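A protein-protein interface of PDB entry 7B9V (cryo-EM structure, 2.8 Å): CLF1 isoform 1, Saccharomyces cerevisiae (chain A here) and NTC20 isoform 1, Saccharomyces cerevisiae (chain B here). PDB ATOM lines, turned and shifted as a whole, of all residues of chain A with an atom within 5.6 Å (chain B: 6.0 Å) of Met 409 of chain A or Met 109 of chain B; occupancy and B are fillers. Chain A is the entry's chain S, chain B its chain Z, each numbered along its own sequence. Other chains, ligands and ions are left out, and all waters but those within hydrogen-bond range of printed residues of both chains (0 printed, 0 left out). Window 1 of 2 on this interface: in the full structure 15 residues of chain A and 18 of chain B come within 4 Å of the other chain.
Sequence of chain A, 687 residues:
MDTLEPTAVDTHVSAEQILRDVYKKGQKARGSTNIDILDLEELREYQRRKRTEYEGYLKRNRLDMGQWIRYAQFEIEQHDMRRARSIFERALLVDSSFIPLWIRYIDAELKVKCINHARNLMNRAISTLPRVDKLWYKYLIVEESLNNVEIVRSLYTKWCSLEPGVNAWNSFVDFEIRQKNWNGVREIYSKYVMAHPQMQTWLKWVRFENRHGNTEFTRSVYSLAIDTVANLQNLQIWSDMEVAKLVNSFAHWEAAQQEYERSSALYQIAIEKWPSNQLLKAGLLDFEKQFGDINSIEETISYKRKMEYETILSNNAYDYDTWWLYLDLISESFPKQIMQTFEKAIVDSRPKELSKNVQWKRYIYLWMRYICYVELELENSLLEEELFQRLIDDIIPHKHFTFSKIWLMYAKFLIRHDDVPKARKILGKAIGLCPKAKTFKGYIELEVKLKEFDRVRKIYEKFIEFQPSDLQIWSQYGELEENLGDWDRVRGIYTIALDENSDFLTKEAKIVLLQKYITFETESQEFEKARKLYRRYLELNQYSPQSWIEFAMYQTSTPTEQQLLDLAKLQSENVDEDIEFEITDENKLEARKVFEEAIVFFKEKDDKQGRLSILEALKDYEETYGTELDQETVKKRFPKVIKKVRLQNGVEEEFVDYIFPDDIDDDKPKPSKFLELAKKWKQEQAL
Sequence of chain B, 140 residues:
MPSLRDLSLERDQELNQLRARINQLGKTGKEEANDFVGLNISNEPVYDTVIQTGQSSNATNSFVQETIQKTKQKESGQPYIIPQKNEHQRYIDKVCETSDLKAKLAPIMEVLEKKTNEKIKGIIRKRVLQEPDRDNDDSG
OE1 of Glu 113 of chain B lies within salt-bridge range of NZ of Lys 412 of chain A (2.8 Å).
Among the printed residues, merely in contact across the chains: Met 368 of chain A with Leu 105 of chain B, Met 368 of chain A with Met 109 of chain B, Cys 372 of chain A with Ile 108 of chain B, Arg 416 of chain A with Leu 112 of chain B, Cys 372 of chain A with Met 109 of chain B and Met 409 of chain A with Met 109 of chain B.
Of the printed residues of chain B, Met 409 of chain A touches Met 109. Of the printed residues of chain A, Met 109 of chain B touches Met 368 (3.7 Å), Cys 372 (3.9 Å) and Met 409 (3.98 Å). Printed residues of chain B within 4 Å of Arg 416 of chain A: Leu 112. Of the printed residues of chain A, Glu 113 of chain B touches Lys 412 (2.8 Å). Of the printed residues of chain B, Cys 372 of chain A touches Ile 108 (3.8 Å) and Met 109 (3.9 Å). Ala 106 of chain B touches none of the printed residues of chain A. Leu 414 of chain A touches none of the printed residues of chain B. The nearest printed residue of chain A that does not touch Met 109 of chain B is Lys 405 of chain A (6.4 Å).
Hydrophobic or aromatic side chains of chain A within 4 Å of the printed part of chain B: Met 368 and Met 409. Hydrophobic or aromatic side chains of chain B within 4 Å of the printed part of chain A: Leu 105, Ile 108, Met 109 and Leu 112. Among the printed residues, 7 pairs touch across the chains. Among the printed residues, Asp or Glu carboxylates within 4 Å of a Lys or Arg side-chain nitrogen of the other chain: Lys 412 of chain A with Glu 113 of chain B.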
ATOM      1  N   MET A 368       7.492  19.320   4.451  1.00  0.00           N
ATOM      2  CA  MET A 368       7.610  18.235   3.471  1.00  0.00           C
ATOM      3  C   MET A 368       8.164  16.961   4.101  1.00  0.00           C
ATOM      4  O   MET A 368       7.683  15.844   3.826  1.00  0.00           O
ATOM      5  CB  MET A 368       8.476  18.699   2.302  1.00  0.00           C
ATOM      6  CG  MET A 368       8.245  17.963   0.993  1.00  0.00           C
ATOM      7  SD  MET A 368       9.144  18.783  -0.341  1.00  0.00           S
ATOM      8  CE  MET A 368       8.320  18.144  -1.796  1.00  0.00           C
ATOM      9  N   ILE A 371       5.185  15.666   6.264  1.00  0.00           N
ATOM     10  CA  ILE A 371       4.261  14.984   5.344  1.00  0.00           C
ATOM     11  C   ILE A 371       4.747  13.576   5.020  1.00  0.00           C
ATOM     12  O   ILE A 371       3.984  12.602   5.107  1.00  0.00           O
ATOM     13  CB  ILE A 371       4.064  15.814   4.059  1.00  0.00           C
ATOM     14  CG1 ILE A 371       3.194  17.027   4.333  1.00  0.00           C
ATOM     15  CG2 ILE A 371       3.397  15.000   2.956  1.00  0.00           C
ATOM     16  CD1 ILE A 371       3.410  18.102   3.328  1.00  0.00           C
ATOM     17  N   CYS A 372       6.016  13.445   4.627  1.00  0.00           N
ATOM     18  CA  CYS A 372       6.489  12.111   4.280  1.00  0.00           C
ATOM     19  C   CYS A 372       6.679  11.238   5.520  1.00  0.00           C
ATOM     20  O   CYS A 372       6.561  10.018   5.402  1.00  0.00           O
ATOM     21  CB  CYS A 372       7.780  12.153   3.470  1.00  0.00           C
ATOM     22  SG  CYS A 372       9.296  12.081   4.434  1.00  0.00           S
ATOM     23  N   PHE A 388      -1.878  19.227   5.353  1.00  0.00           N
ATOM     24  CA  PHE A 388      -2.051  19.917   4.068  1.00  0.00           C
ATOM     25  C   PHE A 388      -3.049  21.076   4.146  1.00  0.00           C
ATOM     26  O   PHE A 388      -2.821  22.120   3.519  1.00  0.00           O
ATOM     27  CB  PHE A 388      -2.480  18.946   2.962  1.00  0.00           C
ATOM     28  CG  PHE A 388      -1.361  18.109   2.355  1.00  0.00           C
ATOM     29  CD1 PHE A 388      -0.334  18.740   1.669  1.00  0.00           C
ATOM     30  CD2 PHE A 388      -1.409  16.718   2.337  1.00  0.00           C
ATOM     31  CE1 PHE A 388       0.659  18.001   1.045  1.00  0.00           C
ATOM     32  CE2 PHE A 388      -0.405  15.972   1.734  1.00  0.00           C
ATOM     33  CZ  PHE A 388       0.628  16.619   1.085  1.00  0.00           C
ATOM     34  N   SER A 404       4.738  25.951  -4.929  1.00  0.00           N
ATOM     35  CA  SER A 404       4.271  24.922  -5.863  1.00  0.00           C
ATOM     36  C   SER A 404       4.467  23.502  -5.337  1.00  0.00           C
ATOM     37  O   SER A 404       3.656  22.612  -5.622  1.00  0.00           O
ATOM     38  CB  SER A 404       4.978  25.091  -7.207  1.00  0.00           C
ATOM     39  OG  SER A 404       6.378  24.917  -7.091  1.00  0.00           O
ATOM     40  N   LYS A 405       5.582  23.274  -4.632  1.00  0.00           N
ATOM     41  CA  LYS A 405       5.968  21.984  -4.054  1.00  0.00           C
ATOM     42  C   LYS A 405       4.887  21.369  -3.163  1.00  0.00           C
ATOM     43  O   LYS A 405       4.521  20.212  -3.368  1.00  0.00           O
ATOM     44  CB  LYS A 405       7.268  22.135  -3.257  1.00  0.00           C
ATOM     45  CG  LYS A 405       8.497  22.603  -4.059  1.00  0.00           C
ATOM     46  CD  LYS A 405       9.735  22.780  -3.168  1.00  0.00           C
ATOM     47  CE  LYS A 405      10.246  21.464  -2.592  1.00  0.00           C
ATOM     48  NZ  LYS A 405      10.867  20.569  -3.605  1.00  0.00           N
ATOM     49  N   ILE A 406       4.193  22.184  -2.364  1.00  0.00           N
ATOM     50  CA  ILE A 406       3.156  21.676  -1.457  1.00  0.00           C
ATOM     51  C   ILE A 406       1.840  21.429  -2.195  1.00  0.00           C
ATOM     52  O   ILE A 406       1.170  20.427  -1.922  1.00  0.00           O
ATOM     53  CB  ILE A 406       2.982  22.630  -0.249  1.00  0.00           C
ATOM     54  CG1 ILE A 406       4.270  22.718   0.570  1.00  0.00           C
ATOM     55  CG2 ILE A 406       1.835  22.209   0.698  1.00  0.00           C
ATOM     56  CD1 ILE A 406       4.708  21.373   1.146  1.00  0.00           C
ATOM     57  N   TRP A 407       1.444  22.314  -3.125  1.00  0.00           N
ATOM     58  CA  TRP A 407       0.257  22.084  -3.969  1.00  0.00           C
ATOM     59  C   TRP A 407       0.401  20.802  -4.791  1.00  0.00           C
ATOM     60  O   TRP A 407      -0.543  20.010  -4.879  1.00  0.00           O
ATOM     61  CB  TRP A 407      -0.024  23.272  -4.894  1.00  0.00           C
ATOM     62  CG  TRP A 407      -0.491  24.520  -4.208  1.00  0.00           C
ATOM     63  CD1 TRP A 407       0.224  25.659  -4.037  1.00  0.00           C
ATOM     64  CD2 TRP A 407      -1.786  24.761  -3.614  1.00  0.00           C
ATOM     65  NE1 TRP A 407      -0.518  26.588  -3.362  1.00  0.00           N
ATOM     66  CE2 TRP A 407      -1.751  26.072  -3.097  1.00  0.00           C
ATOM     67  CE3 TRP A 407      -2.947  24.008  -3.466  1.00  0.00           C
ATOM     68  CZ2 TRP A 407      -2.841  26.643  -2.444  1.00  0.00           C
ATOM     69  CZ3 TRP A 407      -4.027  24.574  -2.823  1.00  0.00           C
ATOM     70  CH2 TRP A 407      -3.966  25.881  -2.322  1.00  0.00           C
ATOM     71  N   LEU A 408       1.533  20.639  -5.485  1.00  0.00           N
ATOM     72  CA  LEU A 408       1.782  19.426  -6.270  1.00  0.00           C
ATOM     73  C   LEU A 408       1.847  18.180  -5.380  1.00  0.00           C
ATOM     74  O   LEU A 408       1.375  17.109  -5.795  1.00  0.00           O
ATOM     75  CB  LEU A 408       3.035  19.578  -7.140  1.00  0.00           C
ATOM     76  CG  LEU A 408       3.008  20.687  -8.195  1.00  0.00           C
ATOM     77  CD1 LEU A 408       4.326  20.746  -8.950  1.00  0.00           C
ATOM     78  CD2 LEU A 408       1.850  20.489  -9.163  1.00  0.00           C
ATOM     79  N   MET A 409       2.459  18.281  -4.182  1.00  0.00           N
ATOM     80  CA  MET A 409       2.407  17.189  -3.194  1.00  0.00           C
ATOM     81  C   MET A 409       0.968  16.843  -2.814  1.00  0.00           C
ATOM     82  O   MET A 409       0.630  15.665  -2.707  1.00  0.00           O
ATOM     83  CB  MET A 409       3.229  17.496  -1.940  1.00  0.00           C
ATOM     84  CG  MET A 409       4.729  17.275  -2.103  1.00  0.00           C
ATOM     85  SD  MET A 409       5.308  15.565  -2.091  1.00  0.00           S
ATOM     86  CE  MET A 409       5.164  15.192  -0.352  1.00  0.00           C
ATOM     87  N   TYR A 410       0.135  17.852  -2.525  1.00  0.00           N
ATOM     88  CA  TYR A 410      -1.273  17.628  -2.156  1.00  0.00           C
ATOM     89  C   TYR A 410      -2.067  16.987  -3.281  1.00  0.00           C
ATOM     90  O   TYR A 410      -2.821  16.031  -3.047  1.00  0.00           O
ATOM     91  CB  TYR A 410      -1.915  18.950  -1.723  1.00  0.00           C
ATOM     92  CG  TYR A 410      -3.311  18.817  -1.134  1.00  0.00           C
ATOM     93  CD1 TYR A 410      -3.589  17.882  -0.162  1.00  0.00           C
ATOM     94  CD2 TYR A 410      -4.306  19.744  -1.457  1.00  0.00           C
ATOM     95  CE1 TYR A 410      -4.850  17.786   0.416  1.00  0.00           C
ATOM     96  CE2 TYR A 410      -5.576  19.668  -0.884  1.00  0.00           C
ATOM     97  CZ  TYR A 410      -5.836  18.684   0.057  1.00  0.00           C
ATOM     98  OH  TYR A 410      -7.077  18.581   0.636  1.00  0.00           O
ATOM     99  N   ALA A 411      -1.955  17.546  -4.484  1.00  0.00           N
ATOM    100  CA  ALA A 411      -2.582  17.004  -5.691  1.00  0.00           C
ATOM    101  C   ALA A 411      -2.180  15.555  -5.959  1.00  0.00           C
ATOM    102  O   ALA A 411      -3.036  14.718  -6.264  1.00  0.00           O
ATOM    103  CB  ALA A 411      -2.236  17.876  -6.895  1.00  0.00           C
ATOM    104  N   LYS A 412      -0.890  15.237  -5.827  1.00  0.00           N
ATOM    105  CA  LYS A 412      -0.448  13.856  -6.003  1.00  0.00           C
ATOM    106  C   LYS A 412      -0.835  12.968  -4.825  1.00  0.00           C
ATOM    107  O   LYS A 412      -1.017  11.759  -5.016  1.00  0.00           O
ATOM    108  CB  LYS A 412       1.061  13.821  -6.237  1.00  0.00           C
ATOM    109  CG  LYS A 412       1.445  14.326  -7.616  1.00  0.00           C
ATOM    110  CD  LYS A 412       2.940  14.255  -7.861  1.00  0.00           C
ATOM    111  CE  LYS A 412       3.267  14.737  -9.265  1.00  0.00           C
ATOM    112  NZ  LYS A 412       4.729  14.743  -9.536  1.00  0.00           N
ATOM    113  N   PHE A 413      -0.879  13.521  -3.607  1.00  0.00           N
ATOM    114  CA  PHE A 413      -1.291  12.774  -2.421  1.00  0.00           C
ATOM    115  C   PHE A 413      -2.732  12.303  -2.548  1.00  0.00           C
ATOM    116  O   PHE A 413      -3.050  11.173  -2.152  1.00  0.00           O
ATOM    117  CB  PHE A 413      -1.114  13.637  -1.159  1.00  0.00           C
ATOM    118  CG  PHE A 413      -2.149  13.371  -0.079  1.00  0.00           C
ATOM    119  CD1 PHE A 413      -2.097  12.219   0.709  1.00  0.00           C
ATOM    120  CD2 PHE A 413      -3.173  14.291   0.155  1.00  0.00           C
ATOM    121  CE1 PHE A 413      -3.070  11.973   1.649  1.00  0.00           C
ATOM    122  CE2 PHE A 413      -4.136  14.050   1.119  1.00  0.00           C
ATOM    123  CZ  PHE A 413      -4.080  12.892   1.871  1.00  0.00           C
ATOM    124  N   LEU A 414      -3.622  13.186  -3.037  1.00  0.00           N
ATOM    125  CA  LEU A 414      -5.068  12.924  -3.093  1.00  0.00           C
ATOM    126  C   LEU A 414      -5.399  11.695  -3.941  1.00  0.00           C
ATOM    127  O   LEU A 414      -6.415  11.032  -3.703  1.00  0.00           O
ATOM    128  CB  LEU A 414      -5.788  14.170  -3.610  1.00  0.00           C
ATOM    129  CG  LEU A 414      -5.969  15.272  -2.559  1.00  0.00           C
ATOM    130  CD1 LEU A 414      -6.352  16.593  -3.200  1.00  0.00           C
ATOM    131  CD2 LEU A 414      -6.995  14.878  -1.517  1.00  0.00           C
ATOM    132  N   ARG A 416      -3.408   8.982  -3.934  1.00  0.00           N
ATOM    133  CA  ARG A 416      -3.203   7.911  -2.962  1.00  0.00           C
ATOM    134  C   ARG A 416      -4.249   7.892  -1.845  1.00  0.00           C
ATOM    135  O   ARG A 416      -4.454   6.833  -1.238  1.00  0.00           O
ATOM    136  CB  ARG A 416      -1.800   8.038  -2.347  1.00  0.00           C
ATOM    137  CG  ARG A 416      -0.653   7.650  -3.281  1.00  0.00           C
ATOM    138  CD  ARG A 416       0.722   7.934  -2.677  1.00  0.00           C
ATOM    139  NE  ARG A 416       1.231   9.226  -3.127  1.00  0.00           N
ATOM    140  CZ  ARG A 416       1.553  10.242  -2.340  1.00  0.00           C
ATOM    141  NH1 ARG A 416       1.446  10.160  -1.025  1.00  0.00           N
ATOM    142  NH2 ARG A 416       2.004  11.367  -2.890  1.00  0.00           N
ATOM    143  N   LEU B 105      15.833  15.044   0.442  1.00  0.00           N
ATOM    144  CA  LEU B 105      14.448  14.573   0.417  1.00  0.00           C
ATOM    145  C   LEU B 105      14.159  13.717  -0.805  1.00  0.00           C
ATOM    146  O   LEU B 105      13.231  12.897  -0.745  1.00  0.00           O
ATOM    147  CB  LEU B 105      13.459  15.729   0.467  1.00  0.00           C
ATOM    148  CG  LEU B 105      13.063  16.332   1.812  1.00  0.00           C
ATOM    149  CD1 LEU B 105      11.900  17.255   1.577  1.00  0.00           C
ATOM    150  CD2 LEU B 105      12.703  15.283   2.852  1.00  0.00           C
ATOM    151  N   ALA B 106      14.884  13.949  -1.917  1.00  0.00           N
ATOM    152  CA  ALA B 106      14.627  13.333  -3.227  1.00  0.00           C
ATOM    153  C   ALA B 106      14.466  11.803  -3.203  1.00  0.00           C
ATOM    154  O   ALA B 106      13.582  11.313  -3.923  1.00  0.00           O
ATOM    155  CB  ALA B 106      15.692  13.801  -4.229  1.00  0.00           C
ATOM    156  N   PRO B 107      15.310  10.985  -2.506  1.00  0.00           N
ATOM    157  CA  PRO B 107      15.071   9.521  -2.520  1.00  0.00           C
ATOM    158  C   PRO B 107      13.731   9.096  -1.920  1.00  0.00           C
ATOM    159  O   PRO B 107      13.197   8.050  -2.304  1.00  0.00           O
ATOM    160  CB  PRO B 107      16.253   8.947  -1.736  1.00  0.00           C
ATOM    161  CG  PRO B 107      17.273   9.940  -1.833  1.00  0.00           C
ATOM    162  CD  PRO B 107      16.597  11.232  -1.798  1.00  0.00           C
ATOM    163  N   ILE B 108      13.176   9.879  -0.992  1.00  0.00           N
ATOM    164  CA  ILE B 108      11.827   9.604  -0.501  1.00  0.00           C
ATOM    165  C   ILE B 108      10.789  10.162  -1.473  1.00  0.00           C
ATOM    166  O   ILE B 108       9.744   9.527  -1.698  1.00  0.00           O
ATOM    167  CB  ILE B 108      11.647  10.187   0.922  1.00  0.00           C
ATOM    168  CG1 ILE B 108      12.728   9.677   1.871  1.00  0.00           C
ATOM    169  CG2 ILE B 108      10.292   9.853   1.517  1.00  0.00           C
ATOM    170  CD1 ILE B 108      12.736  10.401   3.205  1.00  0.00           C
ATOM    171  N   MET B 109      11.045  11.354  -2.040  1.00  0.00           N
ATOM    172  CA  MET B 109      10.089  11.968  -2.960  1.00  0.00           C
ATOM    173  C   MET B 109       9.930  11.134  -4.230  1.00  0.00           C
ATOM    174  O   MET B 109       8.832  11.072  -4.789  1.00  0.00           O
ATOM    175  CB  MET B 109      10.518  13.392  -3.316  1.00  0.00           C
ATOM    176  CG  MET B 109      10.586  14.358  -2.133  1.00  0.00           C
ATOM    177  SD  MET B 109       9.051  14.530  -1.202  1.00  0.00           S
ATOM    178  CE  MET B 109       9.539  13.841   0.378  1.00  0.00           C
ATOM    179  N   GLU B 110      11.010  10.490  -4.702  1.00  0.00           N
ATOM    180  CA  GLU B 110      10.891   9.637  -5.881  1.00  0.00           C
ATOM    181  C   GLU B 110      10.115   8.358  -5.584  1.00  0.00           C
ATOM    182  O   GLU B 110       9.419   7.844  -6.471  1.00  0.00           O
ATOM    183  CB  GLU B 110      12.270   9.280  -6.446  1.00  0.00           C
ATOM    184  CG  GLU B 110      13.086  10.431  -7.037  1.00  0.00           C
ATOM    185  CD  GLU B 110      12.315  11.269  -8.043  1.00  0.00           C
ATOM    186  OE1 GLU B 110      11.652  10.693  -8.933  1.00  0.00           O
ATOM    187  OE2 GLU B 110      12.381  12.512  -7.949  1.00  0.00           O
ATOM    188  N   VAL B 111      10.245   7.817  -4.359  1.00  0.00           N
ATOM    189  CA  VAL B 111       9.434   6.666  -3.958  1.00  0.00           C
ATOM    190  C   VAL B 111       7.962   7.043  -3.915  1.00  0.00           C
ATOM    191  O   VAL B 111       7.100   6.287  -4.392  1.00  0.00           O
ATOM    192  CB  VAL B 111       9.933   6.128  -2.596  1.00  0.00           C
ATOM    193  CG1 VAL B 111       8.905   5.222  -1.896  1.00  0.00           C
ATOM    194  CG2 VAL B 111      11.230   5.367  -2.774  1.00  0.00           C
ATOM    195  N   LEU B 112       7.655   8.240  -3.380  1.00  0.00           N
ATOM    196  CA  LEU B 112       6.265   8.690  -3.370  1.00  0.00           C
ATOM    197  C   LEU B 112       5.753   8.971  -4.775  1.00  0.00           C
ATOM    198  O   LEU B 112       4.564   8.761  -5.051  1.00  0.00           O
ATOM    199  CB  LEU B 112       6.100   9.941  -2.509  1.00  0.00           C
ATOM    200  CG  LEU B 112       6.172   9.739  -1.000  1.00  0.00           C
ATOM    201  CD1 LEU B 112       6.068  11.071  -0.266  1.00  0.00           C
ATOM    202  CD2 LEU B 112       5.062   8.784  -0.597  1.00  0.00           C
ATOM    203  N   GLU B 113       6.644   9.462  -5.651  1.00  0.00           N
ATOM    204  CA  GLU B 113       6.318   9.691  -7.052  1.00  0.00           C
ATOM    205  C   GLU B 113       5.922   8.389  -7.738  1.00  0.00           C
ATOM    206  O   GLU B 113       4.907   8.325  -8.450  1.00  0.00           O
ATOM    207  CB  GLU B 113       7.514  10.325  -7.768  1.00  0.00           C
ATOM    208  CG  GLU B 113       7.384  10.491  -9.295  1.00  0.00           C
ATOM    209  CD  GLU B 113       6.209  11.368  -9.779  1.00  0.00           C
ATOM    210  OE1 GLU B 113       5.640  12.181  -9.012  1.00  0.00           O
ATOM    211  OE2 GLU B 113       5.837  11.233 -10.963  1.00  0.00           O
ATOM    212  N   LYS B 114       6.752   7.345  -7.562  1.00  0.00           N
ATOM    213  CA  LYS B 114       6.469   6.077  -8.221  1.00  0.00           C
ATOM    214  C   LYS B 114       5.232   5.409  -7.631  1.00  0.00           C
ATOM    215  O   LYS B 114       4.467   4.803  -8.383  1.00  0.00           O
ATOM    216  CB  LYS B 114       7.703   5.146  -8.199  1.00  0.00           C
ATOM    217  CG  LYS B 114       7.978   4.317  -6.933  1.00  0.00           C
ATOM    218  CD  LYS B 114       9.337   3.619  -6.953  1.00  0.00           C
ATOM    219  CE  LYS B 114       9.405   2.526  -8.016  1.00  0.00           C
ATOM    220  NZ  LYS B 114       8.458   1.404  -7.743  1.00  0.00           N
